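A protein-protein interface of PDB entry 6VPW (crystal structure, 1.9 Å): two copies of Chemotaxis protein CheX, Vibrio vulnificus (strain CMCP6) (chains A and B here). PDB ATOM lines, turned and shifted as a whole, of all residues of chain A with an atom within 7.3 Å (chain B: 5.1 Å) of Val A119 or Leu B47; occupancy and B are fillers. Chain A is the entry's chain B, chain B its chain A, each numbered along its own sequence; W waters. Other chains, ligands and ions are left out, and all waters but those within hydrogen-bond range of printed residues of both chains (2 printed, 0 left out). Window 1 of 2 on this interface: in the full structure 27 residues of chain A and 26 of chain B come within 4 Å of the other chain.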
ATOM      1  N   SER A  45      10.980   1.489  20.939  1.00  0.00           N
ATOM      2  CA  SER A  45       9.984   1.219  19.877  1.00  0.00           C
ATOM      3  C   SER A  45       9.470  -0.215  19.968  1.00  0.00           C
ATOM      4  O   SER A  45      10.280  -1.140  20.272  1.00  0.00           O
ATOM      5  CB  SER A  45      10.576   1.451  18.505  1.00  0.00           C
ATOM      6  OG  SER A  45      10.934   2.809  18.308  1.00  0.00           O
ATOM      7  N   GLY A  46       8.163  -0.363  19.744  1.00  0.00           N
ATOM      8  CA  GLY A  46       7.492  -1.659  19.619  1.00  0.00           C
ATOM      9  C   GLY A  46       7.196  -1.901  18.152  1.00  0.00           C
ATOM     10  O   GLY A  46       6.622  -0.989  17.510  1.00  0.00           O
ATOM     11  N   LEU A  47       7.602  -3.052  17.622  1.00  0.00           N
ATOM     12  CA  LEU A  47       7.405  -3.333  16.182  1.00  0.00           C
ATOM     13  C   LEU A  47       6.704  -4.686  16.034  1.00  0.00           C
ATOM     14  O   LEU A  47       7.067  -5.658  16.763  1.00  0.00           O
ATOM     15  CB  LEU A  47       8.758  -3.307  15.454  1.00  0.00           C
ATOM     16  CG  LEU A  47       9.551  -1.998  15.551  1.00  0.00           C
ATOM     17  CD1 LEU A  47      10.506  -1.999  16.736  1.00  0.00           C
ATOM     18  CD2 LEU A  47      10.341  -1.738  14.278  1.00  0.00           C
ATOM     19  N   ILE A  48       5.739  -4.744  15.125  1.00  0.00           N
ATOM     20  CA  ILE A  48       5.013  -6.022  14.907  1.00  0.00           C
ATOM     21  C   ILE A  48       4.662  -6.181  13.429  1.00  0.00           C
ATOM     22  O   ILE A  48       4.250  -5.192  12.774  1.00  0.00           O
ATOM     23  CB  ILE A  48       3.770  -6.106  15.816  1.00  0.00           C
ATOM     24  CG1 ILE A  48       3.167  -7.510  15.791  1.00  0.00           C
ATOM     25  CG2 ILE A  48       2.753  -5.042  15.443  1.00  0.00           C
ATOM     26  CD1 ILE A  48       2.275  -7.814  16.970  1.00  0.00           C
ATOM     27  N   GLY A  49       4.821  -7.400  12.928  1.00  0.00           N
ATOM     28  CA  GLY A  49       4.430  -7.702  11.545  1.00  0.00           C
ATOM     29  C   GLY A  49       2.983  -8.177  11.477  1.00  0.00           C
ATOM     30  O   GLY A  49       2.487  -8.751  12.464  1.00  0.00           O
ATOM     31  N   SER A  58       3.525  -3.991   8.426  1.00  0.00           N
ATOM     32  CA  SER A  58       4.152  -3.892   9.757  1.00  0.00           C
ATOM     33  C   SER A  58       3.717  -2.594  10.412  1.00  0.00           C
ATOM     34  O   SER A  58       3.302  -1.663   9.696  1.00  0.00           O
ATOM     35  CB  SER A  58       5.668  -3.966   9.645  1.00  0.00           C
ATOM     36  OG  SER A  58       6.125  -3.041   8.650  1.00  0.00           O
ATOM     37  N   MET A  59       3.815  -2.561  11.733  1.00  0.00           N
ATOM     38  CA  MET A  59       3.467  -1.329  12.443  1.00  0.00           C
ATOM     39  C   MET A  59       4.537  -1.110  13.508  1.00  0.00           C
ATOM     40  O   MET A  59       5.082  -2.125  14.029  1.00  0.00           O
ATOM     41  CB  MET A  59       2.076  -1.454  13.066  1.00  0.00           C
ATOM     42  CG  MET A  59       1.602  -0.211  13.785  1.00  0.00           C
ATOM     43  SD  MET A  59       2.090  -0.099  15.527  1.00  0.00           S
ATOM     44  CE  MET A  59       1.124  -1.415  16.265  1.00  0.00           C
ATOM     45  N   ILE A  61       5.429   1.532  17.037  1.00  0.00           N
ATOM     46  CA  ILE A  61       5.099   2.649  17.963  1.00  0.00           C
ATOM     47  C   ILE A  61       6.437   3.057  18.581  1.00  0.00           C
ATOM     48  O   ILE A  61       7.077   2.178  19.218  1.00  0.00           O
ATOM     49  CB  ILE A  61       4.081   2.246  19.052  1.00  0.00           C
ATOM     50  CG1 ILE A  61       2.831   1.584  18.476  1.00  0.00           C
ATOM     51  CG2 ILE A  61       3.717   3.457  19.911  1.00  0.00           C
ATOM     52  CD1 ILE A  61       1.946   0.944  19.524  1.00  0.00           C
ATOM     53  N   THR A  88      10.604  -2.335  28.544  1.00  0.00           N
ATOM     54  CA  THR A  88      10.488  -3.001  27.216  1.00  0.00           C
ATOM     55  C   THR A  88       9.296  -3.960  27.239  1.00  0.00           C
ATOM     56  O   THR A  88       8.564  -3.997  26.231  1.00  0.00           O
ATOM     57  CB  THR A  88      11.791  -3.689  26.782  1.00  0.00           C
ATOM     58  OG1 THR A  88      12.087  -4.730  27.713  1.00  0.00           O
ATOM     59  CG2 THR A  88      12.950  -2.723  26.658  1.00  0.00           C
ATOM     60  N   VAL A  91       6.251  -1.876  26.655  1.00  0.00           N
ATOM     61  CA  VAL A  91       6.115  -1.434  25.234  1.00  0.00           C
ATOM     62  C   VAL A  91       5.648  -2.630  24.394  1.00  0.00           C
ATOM     63  O   VAL A  91       4.760  -2.442  23.541  1.00  0.00           O
ATOM     64  CB  VAL A  91       7.409  -0.784  24.712  1.00  0.00           C
ATOM     65  CG1 VAL A  91       7.368  -0.537  23.211  1.00  0.00           C
ATOM     66  CG2 VAL A  91       7.690   0.518  25.459  1.00  0.00           C
ATOM     67  N   GLY A  92       6.167  -3.824  24.675  1.00  0.00           N
ATOM     68  CA  GLY A  92       5.716  -5.030  23.954  1.00  0.00           C
ATOM     69  C   GLY A  92       4.227  -5.282  24.138  1.00  0.00           C
ATOM     70  O   GLY A  92       3.549  -5.540  23.137  1.00  0.00           O
ATOM     71  N   THR A  95       2.124  -2.634  22.286  1.00  0.00           N
ATOM     72  CA  THR A  95       2.122  -2.951  20.834  1.00  0.00           C
ATOM     73  C   THR A  95       1.064  -4.022  20.526  1.00  0.00           C
ATOM     74  O   THR A  95       0.298  -3.821  19.554  1.00  0.00           O
ATOM     75  CB  THR A  95       3.518  -3.380  20.385  1.00  0.00           C
ATOM     76  OG1 THR A  95       4.391  -2.323  20.773  1.00  0.00           O
ATOM     77  CG2 THR A  95       3.611  -3.642  18.901  1.00  0.00           C
ATOM     78  N   THR A 117       4.534 -11.639  16.446  1.00  0.00           N
ATOM     79  CA  THR A 117       4.876 -11.372  17.867  1.00  0.00           C
ATOM     80  C   THR A 117       5.678 -10.080  17.879  1.00  0.00           C
ATOM     81  O   THR A 117       6.420  -9.808  16.941  1.00  0.00           O
ATOM     82  CB  THR A 117       5.655 -12.535  18.501  1.00  0.00           C
ATOM     83  OG1 THR A 117       6.840 -12.717  17.722  1.00  0.00           O
ATOM     84  CG2 THR A 117       4.864 -13.819  18.556  1.00  0.00           C
ATOM     85  N   PRO A 118       5.530  -9.229  18.915  1.00  0.00           N
ATOM     86  CA  PRO A 118       6.224  -7.952  18.940  1.00  0.00           C
ATOM     87  C   PRO A 118       7.720  -8.064  19.247  1.00  0.00           C
ATOM     88  O   PRO A 118       8.155  -9.012  19.891  1.00  0.00           O
ATOM     89  CB  PRO A 118       5.515  -7.144  20.037  1.00  0.00           C
ATOM     90  CG  PRO A 118       4.806  -8.163  20.904  1.00  0.00           C
ATOM     91  CD  PRO A 118       4.663  -9.432  20.078  1.00  0.00           C
ATOM     92  N   VAL A 119       8.453  -7.100  18.716  1.00  0.00           N
ATOM     93  CA  VAL A 119       9.907  -6.929  18.973  1.00  0.00           C
ATOM     94  C   VAL A 119      10.086  -5.518  19.554  1.00  0.00           C
ATOM     95  O   VAL A 119       9.450  -4.596  19.044  1.00  0.00           O
ATOM     96  CB  VAL A 119      10.729  -7.132  17.693  1.00  0.00           C
ATOM     97  CG1 VAL A 119      12.222  -7.112  17.995  1.00  0.00           C
ATOM     98  CG2 VAL A 119      10.345  -8.425  16.994  1.00  0.00           C
ATOM     99  N   VAL A 120      10.900  -5.373  20.593  1.00  0.00           N
ATOM    100  CA  VAL A 120      11.101  -4.030  21.206  1.00  0.00           C
ATOM    101  C   VAL A 120      12.563  -3.642  21.032  1.00  0.00           C
ATOM    102  O   VAL A 120      13.450  -4.468  21.342  1.00  0.00           O
ATOM    103  CB  VAL A 120      10.667  -3.986  22.679  1.00  0.00           C
ATOM    104  CG1 VAL A 120      10.945  -2.619  23.301  1.00  0.00           C
ATOM    105  CG2 VAL A 120       9.197  -4.353  22.836  1.00  0.00           C
ATOM    106  N   VAL A 121      12.776  -2.446  20.488  1.00  0.00           N
ATOM    107  CA  VAL A 121      14.137  -1.890  20.291  1.00  0.00           C
ATOM    108  C   VAL A 121      14.345  -0.743  21.282  1.00  0.00           C
ATOM    109  O   VAL A 121      13.436   0.096  21.393  1.00  0.00           O
ATOM    110  CB  VAL A 121      14.317  -1.416  18.842  1.00  0.00           C
ATOM    111  CG1 VAL A 121      15.666  -0.745  18.659  1.00  0.00           C
ATOM    112  CG2 VAL A 121      14.153  -2.574  17.869  1.00  0.00           C
ATOM    113  N   SER B  45      19.672  -3.155  12.471  1.00  0.00           N
ATOM    114  CA  SER B  45      18.958  -4.448  12.574  1.00  0.00           C
ATOM    115  C   SER B  45      17.804  -4.518  11.579  1.00  0.00           C
ATOM    116  O   SER B  45      17.159  -3.459  11.325  1.00  0.00           O
ATOM    117  CB  SER B  45      18.403  -4.655  13.954  1.00  0.00           C
ATOM    118  OG  SER B  45      19.410  -4.608  14.941  1.00  0.00           O
ATOM    119  N   GLY B  46      17.598  -5.711  11.028  1.00  0.00           N
ATOM    120  CA  GLY B  46      16.414  -6.065  10.226  1.00  0.00           C
ATOM    121  C   GLY B  46      15.489  -6.898  11.102  1.00  0.00           C
ATOM    122  O   GLY B  46      16.002  -7.794  11.827  1.00  0.00           O
ATOM    123  N   LEU B  47      14.194  -6.575  11.119  1.00  0.00           N
ATOM    124  CA  LEU B  47      13.193  -7.253  11.992  1.00  0.00           C
ATOM    125  C   LEU B  47      12.024  -7.690  11.112  1.00  0.00           C
ATOM    126  O   LEU B  47      11.583  -6.855  10.269  1.00  0.00           O
ATOM    127  CB  LEU B  47      12.663  -6.278  13.051  1.00  0.00           C
ATOM    128  CG  LEU B  47      13.612  -5.850  14.168  1.00  0.00           C
ATOM    129  CD1 LEU B  47      14.780  -5.039  13.639  1.00  0.00           C
ATOM    130  CD2 LEU B  47      12.850  -5.038  15.204  1.00  0.00           C
ATOM    131  N   ILE B  48      11.538  -8.918  11.293  1.00  0.00           N
ATOM    132  CA  ILE B  48      10.399  -9.364  10.446  1.00  0.00           C
ATOM    133  C   ILE B  48       9.508 -10.313  11.248  1.00  0.00           C
ATOM    134  O   ILE B  48      10.025 -11.162  11.984  1.00  0.00           O
ATOM    135  CB  ILE B  48      10.915  -9.983   9.134  1.00  0.00           C
ATOM    136  CG1 ILE B  48       9.779 -10.162   8.121  1.00  0.00           C
ATOM    137  CG2 ILE B  48      11.670 -11.277   9.391  1.00  0.00           C
ATOM    138  CD1 ILE B  48      10.250 -10.461   6.706  1.00  0.00           C
ATOM    139  N   GLY B  49       8.199 -10.158  11.085  1.00  0.00           N
ATOM    140  CA  GLY B  49       7.250 -11.053  11.764  1.00  0.00           C
ATOM    141  C   GLY B  49       6.889 -12.207  10.858  1.00  0.00           C
ATOM    142  O   GLY B  49       6.945 -12.051   9.610  1.00  0.00           O
ATOM    143  N   SER B  58       8.883 -14.079  15.446  1.00  0.00           N
ATOM    144  CA  SER B  58       9.655 -12.949  14.876  1.00  0.00           C
ATOM    145  C   SER B  58      11.130 -13.329  14.785  1.00  0.00           C
ATOM    146  O   SER B  58      11.567 -14.223  15.521  1.00  0.00           O
ATOM    147  CB  SER B  58       9.477 -11.695  15.702  1.00  0.00           C
ATOM    148  OG  SER B  58       9.757 -11.950  17.088  1.00  0.00           O
ATOM    149  N   MET B  59      11.826 -12.688  13.858  1.00  0.00           N
ATOM    150  CA  MET B  59      13.281 -12.880  13.693  1.00  0.00           C
ATOM    151  C   MET B  59      13.928 -11.493  13.544  1.00  0.00           C
ATOM    152  O   MET B  59      13.296 -10.585  12.938  1.00  0.00           O
ATOM    153  CB  MET B  59      13.552 -13.762  12.472  1.00  0.00           C
ATOM    154  CG  MET B  59      15.010 -14.109  12.285  1.00  0.00           C
ATOM    155  SD  MET B  59      15.832 -12.929  11.208  1.00  0.00           S
ATOM    156  CE  MET B  59      15.427 -13.627   9.608  1.00  0.00           C
ATOM    157  N   SER B  60      15.109 -11.322  14.136  1.00  0.00           N
ATOM    158  CA  SER B  60      15.896 -10.083  13.951  1.00  0.00           C
ATOM    159  C   SER B  60      17.337 -10.476  13.600  1.00  0.00           C
ATOM    160  O   SER B  60      17.795 -11.544  14.051  1.00  0.00           O
ATOM    161  CB  SER B  60      15.848  -9.178  15.160  1.00  0.00           C
ATOM    162  OG  SER B  60      16.303  -9.848  16.327  1.00  0.00           O
ATOM    163  N   THR B  95      17.430  -9.355   5.273  1.00  0.00           N
ATOM    164  CA  THR B  95      16.407  -9.925   6.195  1.00  0.00           C
ATOM    165  C   THR B  95      15.372 -10.736   5.388  1.00  0.00           C
ATOM    166  O   THR B  95      15.036 -11.840   5.816  1.00  0.00           O
ATOM    167  CB  THR B  95      15.759  -8.811   7.031  1.00  0.00           C
ATOM    168  OG1 THR B  95      16.785  -8.089   7.721  1.00  0.00           O
ATOM    169  CG2 THR B  95      14.729  -9.331   8.014  1.00  0.00           C
ATOM    170  N   THR B 117       6.430  -7.644   6.471  1.00  0.00           N
ATOM    171  CA  THR B 117       7.397  -6.791   5.751  1.00  0.00           C
ATOM    172  C   THR B 117       8.525  -6.506   6.731  1.00  0.00           C
ATOM    173  O   THR B 117       8.301  -6.390   7.934  1.00  0.00           O
ATOM    174  CB  THR B 117       6.700  -5.540   5.198  1.00  0.00           C
ATOM    175  OG1 THR B 117       6.115  -4.867   6.308  1.00  0.00           O
ATOM    176  CG2 THR B 117       5.625  -5.872   4.193  1.00  0.00           C
ATOM    177  N   PRO B 118       9.779  -6.429   6.254  1.00  0.00           N
ATOM    178  CA  PRO B 118      10.883  -6.138   7.148  1.00  0.00           C
ATOM    179  C   PRO B 118      10.867  -4.661   7.574  1.00  0.00           C
ATOM    180  O   PRO B 118      10.368  -3.786   6.841  1.00  0.00           O
ATOM    181  CB  PRO B 118      12.132  -6.500   6.343  1.00  0.00           C
ATOM    182  CG  PRO B 118      11.709  -6.465   4.891  1.00  0.00           C
ATOM    183  CD  PRO B 118      10.195  -6.591   4.852  1.00  0.00           C
ATOM    184  N   VAL B 119      11.357  -4.443   8.786  1.00  0.00           N
ATOM    185  CA  VAL B 119      11.536  -3.095   9.372  1.00  0.00           C
ATOM    186  C   VAL B 119      13.017  -2.992   9.730  1.00  0.00           C
ATOM    187  O   VAL B 119      13.570  -3.986  10.250  1.00  0.00           O
ATOM    188  CB  VAL B 119      10.631  -2.848  10.589  1.00  0.00           C
ATOM    189  CG1 VAL B 119      10.720  -1.390  11.034  1.00  0.00           C
ATOM    190  CG2 VAL B 119       9.187  -3.204  10.295  1.00  0.00           C
ATOM    191  N   VAL B 120      13.643  -1.869   9.398  1.00  0.00           N
ATOM    192  CA  VAL B 120      15.089  -1.710   9.705  1.00  0.00           C
ATOM    193  C   VAL B 120      15.275  -0.601  10.737  1.00  0.00           C
ATOM    194  O   VAL B 120      14.738   0.517  10.534  1.00  0.00           O
ATOM    195  CB  VAL B 120      15.904  -1.443   8.438  1.00  0.00           C
ATOM    196  CG1 VAL B 120      17.382  -1.237   8.756  1.00  0.00           C
ATOM    197  CG2 VAL B 120      15.707  -2.563   7.438  1.00  0.00           C
ATOM    198  N   VAL B 121      16.022  -0.922  11.794  1.00  0.00           N
ATOM    199  CA  VAL B 121      16.306   0.025  12.905  1.00  0.00           C
ATOM    200  C   VAL B 121      17.780   0.401  12.846  1.00  0.00           C
ATOM    201  O   VAL B 121      18.607  -0.530  12.674  1.00  0.00           O
ATOM    202  CB  VAL B 121      15.961  -0.587  14.274  1.00  0.00           C
ATOM    203  CG1 VAL B 121      16.510   0.260  15.410  1.00  0.00           C
ATOM    204  CG2 VAL B 121      14.463  -0.801  14.421  1.00  0.00           C
ATOM    205  N   ILE B 128      17.837  -5.247  21.201  1.00  0.00           N
ATOM    206  CA  ILE B 128      16.576  -5.863  20.705  1.00  0.00           C
ATOM    207  C   ILE B 128      16.070  -6.864  21.740  1.00  0.00           C
ATOM    208  O   ILE B 128      16.894  -7.587  22.334  1.00  0.00           O
ATOM    209  CB  ILE B 128      16.814  -6.516  19.332  1.00  0.00           C
ATOM    210  CG1 ILE B 128      17.184  -5.449  18.299  1.00  0.00           C
ATOM    211  CG2 ILE B 128      15.612  -7.347  18.891  1.00  0.00           C
ATOM    212  CD1 ILE B 128      17.220  -5.943  16.881  1.00  0.00           C
ATOM    213  N   ARG B 129      14.761  -6.878  21.966  1.00  0.00           N
ATOM    214  CA  ARG B 129      14.159  -7.839  22.917  1.00  0.00           C
ATOM    215  C   ARG B 129      12.875  -8.374  22.294  1.00  0.00           C
ATOM    216  O   ARG B 129      11.913  -7.588  22.135  1.00  0.00           O
ATOM    217  CB  ARG B 129      13.913  -7.202  24.286  1.00  0.00           C
ATOM    218  CG  ARG B 129      15.186  -6.694  24.947  1.00  0.00           C
ATOM    219  CD  ARG B 129      15.020  -6.421  26.425  1.00  0.00           C
ATOM    220  NE  ARG B 129      16.175  -5.718  26.972  1.00  0.00           N
ATOM    221  CZ  ARG B 129      16.480  -5.644  28.266  1.00  0.00           C
ATOM    222  NH1 ARG B 129      15.735  -6.259  29.167  1.00  0.00           N
ATOM    223  NH2 ARG B 129      17.550  -4.973  28.655  1.00  0.00           N
ATOM    224  N   HIS B 130      12.910  -9.640  21.885  1.00  0.00           N
ATOM    225  CA  HIS B 130      11.693 -10.295  21.362  1.00  0.00           C
ATOM    226  C   HIS B 130      10.756 -10.556  22.535  1.00  0.00           C
ATOM    227  O   HIS B 130      11.247 -10.850  23.637  1.00  0.00           O
ATOM    228  CB  HIS B 130      12.069 -11.568  20.613  1.00  0.00           C
ATOM    229  CG  HIS B 130      12.785 -11.285  19.340  1.00  0.00           C
ATOM    230  ND1 HIS B 130      12.189 -11.472  18.118  1.00  0.00           N
ATOM    231  CD2 HIS B 130      14.021 -10.792  19.095  1.00  0.00           C
ATOM    232  CE1 HIS B 130      13.034 -11.132  17.166  1.00  0.00           C
ATOM    233  NE2 HIS B 130      14.161 -10.698  17.742  1.00  0.00           N
ATOM    234  N   LYS B 131       9.457 -10.418  22.304  1.00  0.00           N
ATOM    235  CA  LYS B 131       8.463 -10.722  23.359  1.00  0.00           C
ATOM    236  C   LYS B 131       7.540 -11.793  22.786  1.00  0.00           C
ATOM    237  O   LYS B 131       6.625 -11.427  22.045  1.00  0.00           O
ATOM    238  CB  LYS B 131       7.713  -9.447  23.765  1.00  0.00           C
ATOM    239  CG  LYS B 131       8.589  -8.237  24.076  1.00  0.00           C
ATOM    240  CD  LYS B 131       9.453  -8.372  25.328  1.00  0.00           C
ATOM    241  CE  LYS B 131      10.459  -7.243  25.475  1.00  0.00           C
ATOM    242  NZ  LYS B 131      11.178  -7.287  26.775  1.00  0.00           N
HETATM  243  O   HOH W   1       8.517 -11.574  19.419  1.00  0.00           O
HETATM  244  O   HOH W   2       7.889  -3.006   6.362  1.00  0.00           O
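OG of Ser B58 is in hydrogen-bond range of OG1 of Thr A117, 3.1 Å away. OG1 of Thr B117 sits at hydrogen-bond distance from OG of Ser A58 (3.0 Å). The backbone carbonyl oxygen (O) of Val A120 lies within hydrogen-bond range of the backbone NH (N) of Arg B129 (2.8 Å). NZ of Lys B131 sits at hydrogen-bond distance from OG1 of Thr A88, 2.9 Å away. O of Pro A118 is in hydrogen-bond range of N of Lys B131 (3.1 Å).
O of Ser B45 sits at hydrogen-bond distance from N of Val B121, 2.8 Å away. N of Leu B47 lies within hydrogen-bond range of O of Val B119 (2.8 Å). OG of Ser B58 sits at hydrogen-bond distance from ND1 of His B130, at 2.7 Å. NE2 of His B130 lies within hydrogen-bond range of OG of Ser B60, 2.7 Å away. The backbone carbonyl oxygen (O) of Ser A45 sits at hydrogen-bond distance from the backbone NH (N) of Val A121 (2.8 Å). O of Leu A47 is in hydrogen-bond range of N of Val A119.
Among the printed residues, pairs that only touch across the chains: Leu A47 with Val B119 (3.3 Å), Ser A58 with Val B119 (3.5 Å), Thr A88 with Arg B129 (3.6 Å), Thr A117 with Lys B131 (3.8 Å), Val A119 with Leu B47 (3.5 Å), Val A119 with Ser B58 (3.6 Å), Val A119 with Ile B128 (3.5 Å), Val A119 with Arg B129 (3.8 Å), Val A119 with His B130 (3.7 Å), Val A120 with Ile B128 (3.5 Å), Val A121 with Leu B47 (3.9 Å) and Val A121 with Val B121 (3.5 Å).
Of the printed residues of chain B, Val A119 touches Leu B47, Ser B58, Ile B128, Arg B129 and His B130. Leu B47 touches just these residues of chain A: Val A119 and Val A121. Printed residues of chain A within 4 Å of Arg B129: Thr A88 (3.6 Å), Val A119 (3.8 Å) and Val A120 (2.8 Å). Of the printed residues of chain A, Thr B117 touches Ser A58. Of the printed residues of chain B, Ser A58 touches Thr B117 (3.0 Å) and Val B119 (3.5 Å). Of the printed residues of chain A, His B130 touches Val A119 (3.7 Å). Of the printed residues of chain A, Lys B131 touches Thr A88, Thr A117 and Pro A118. The nearest residue of chain B that does not touch Val A119 is Lys B131 (4.8 Å). The nearest printed residue of chain B that does not touch Thr A117 is Gly B49 (5.4 Å).
Hydrophobic or aromatic side chains of chain A within 4 Å of the printed part of chain B: Leu A47, Pro A118, Val A119, Val A120 and Val A121. Among the printed residues, no Asp or Glu carboxylate lies within 4 Å of a Lys or Arg side-chain nitrogen of the other chain.
Ser A58 touches Thr B117, and with the chains exchanged Thr A117 touches Ser B58. Ser A58 touches Val B119, and with the chains exchanged Val A119 touches Ser B58. Val A121 touches Leu B47, but with the chains exchanged Leu A47 does not touch Val B121 (4.2 Å). Val A121 touches its own counterpart, Val B121. Positions printed for both chains: 45, 46, 47, 48, 49, 58, 59, 95, 117, 118, 119, 120 and 121.
Water W2 lies within hydrogen-bond range of the side-chain hydroxyl (OG1) of Thr B117 (2.6 Å), the backbone carbonyl oxygen (O) of Pro B118 (2.6 Å) and the side-chain hydroxyl (OG) of Ser A58 (2.9 Å). Water W1 lies within hydrogen-bond range of the backbone carbonyl oxygen of Pro A118 (2.6 Å), the side-chain hydroxyl of Thr A117 (2.6 Å), the side-chain hydroxyl of Ser B58 (2.7 Å) and the backbone carbonyl oxygen of Lys B131 (3.2 Å).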
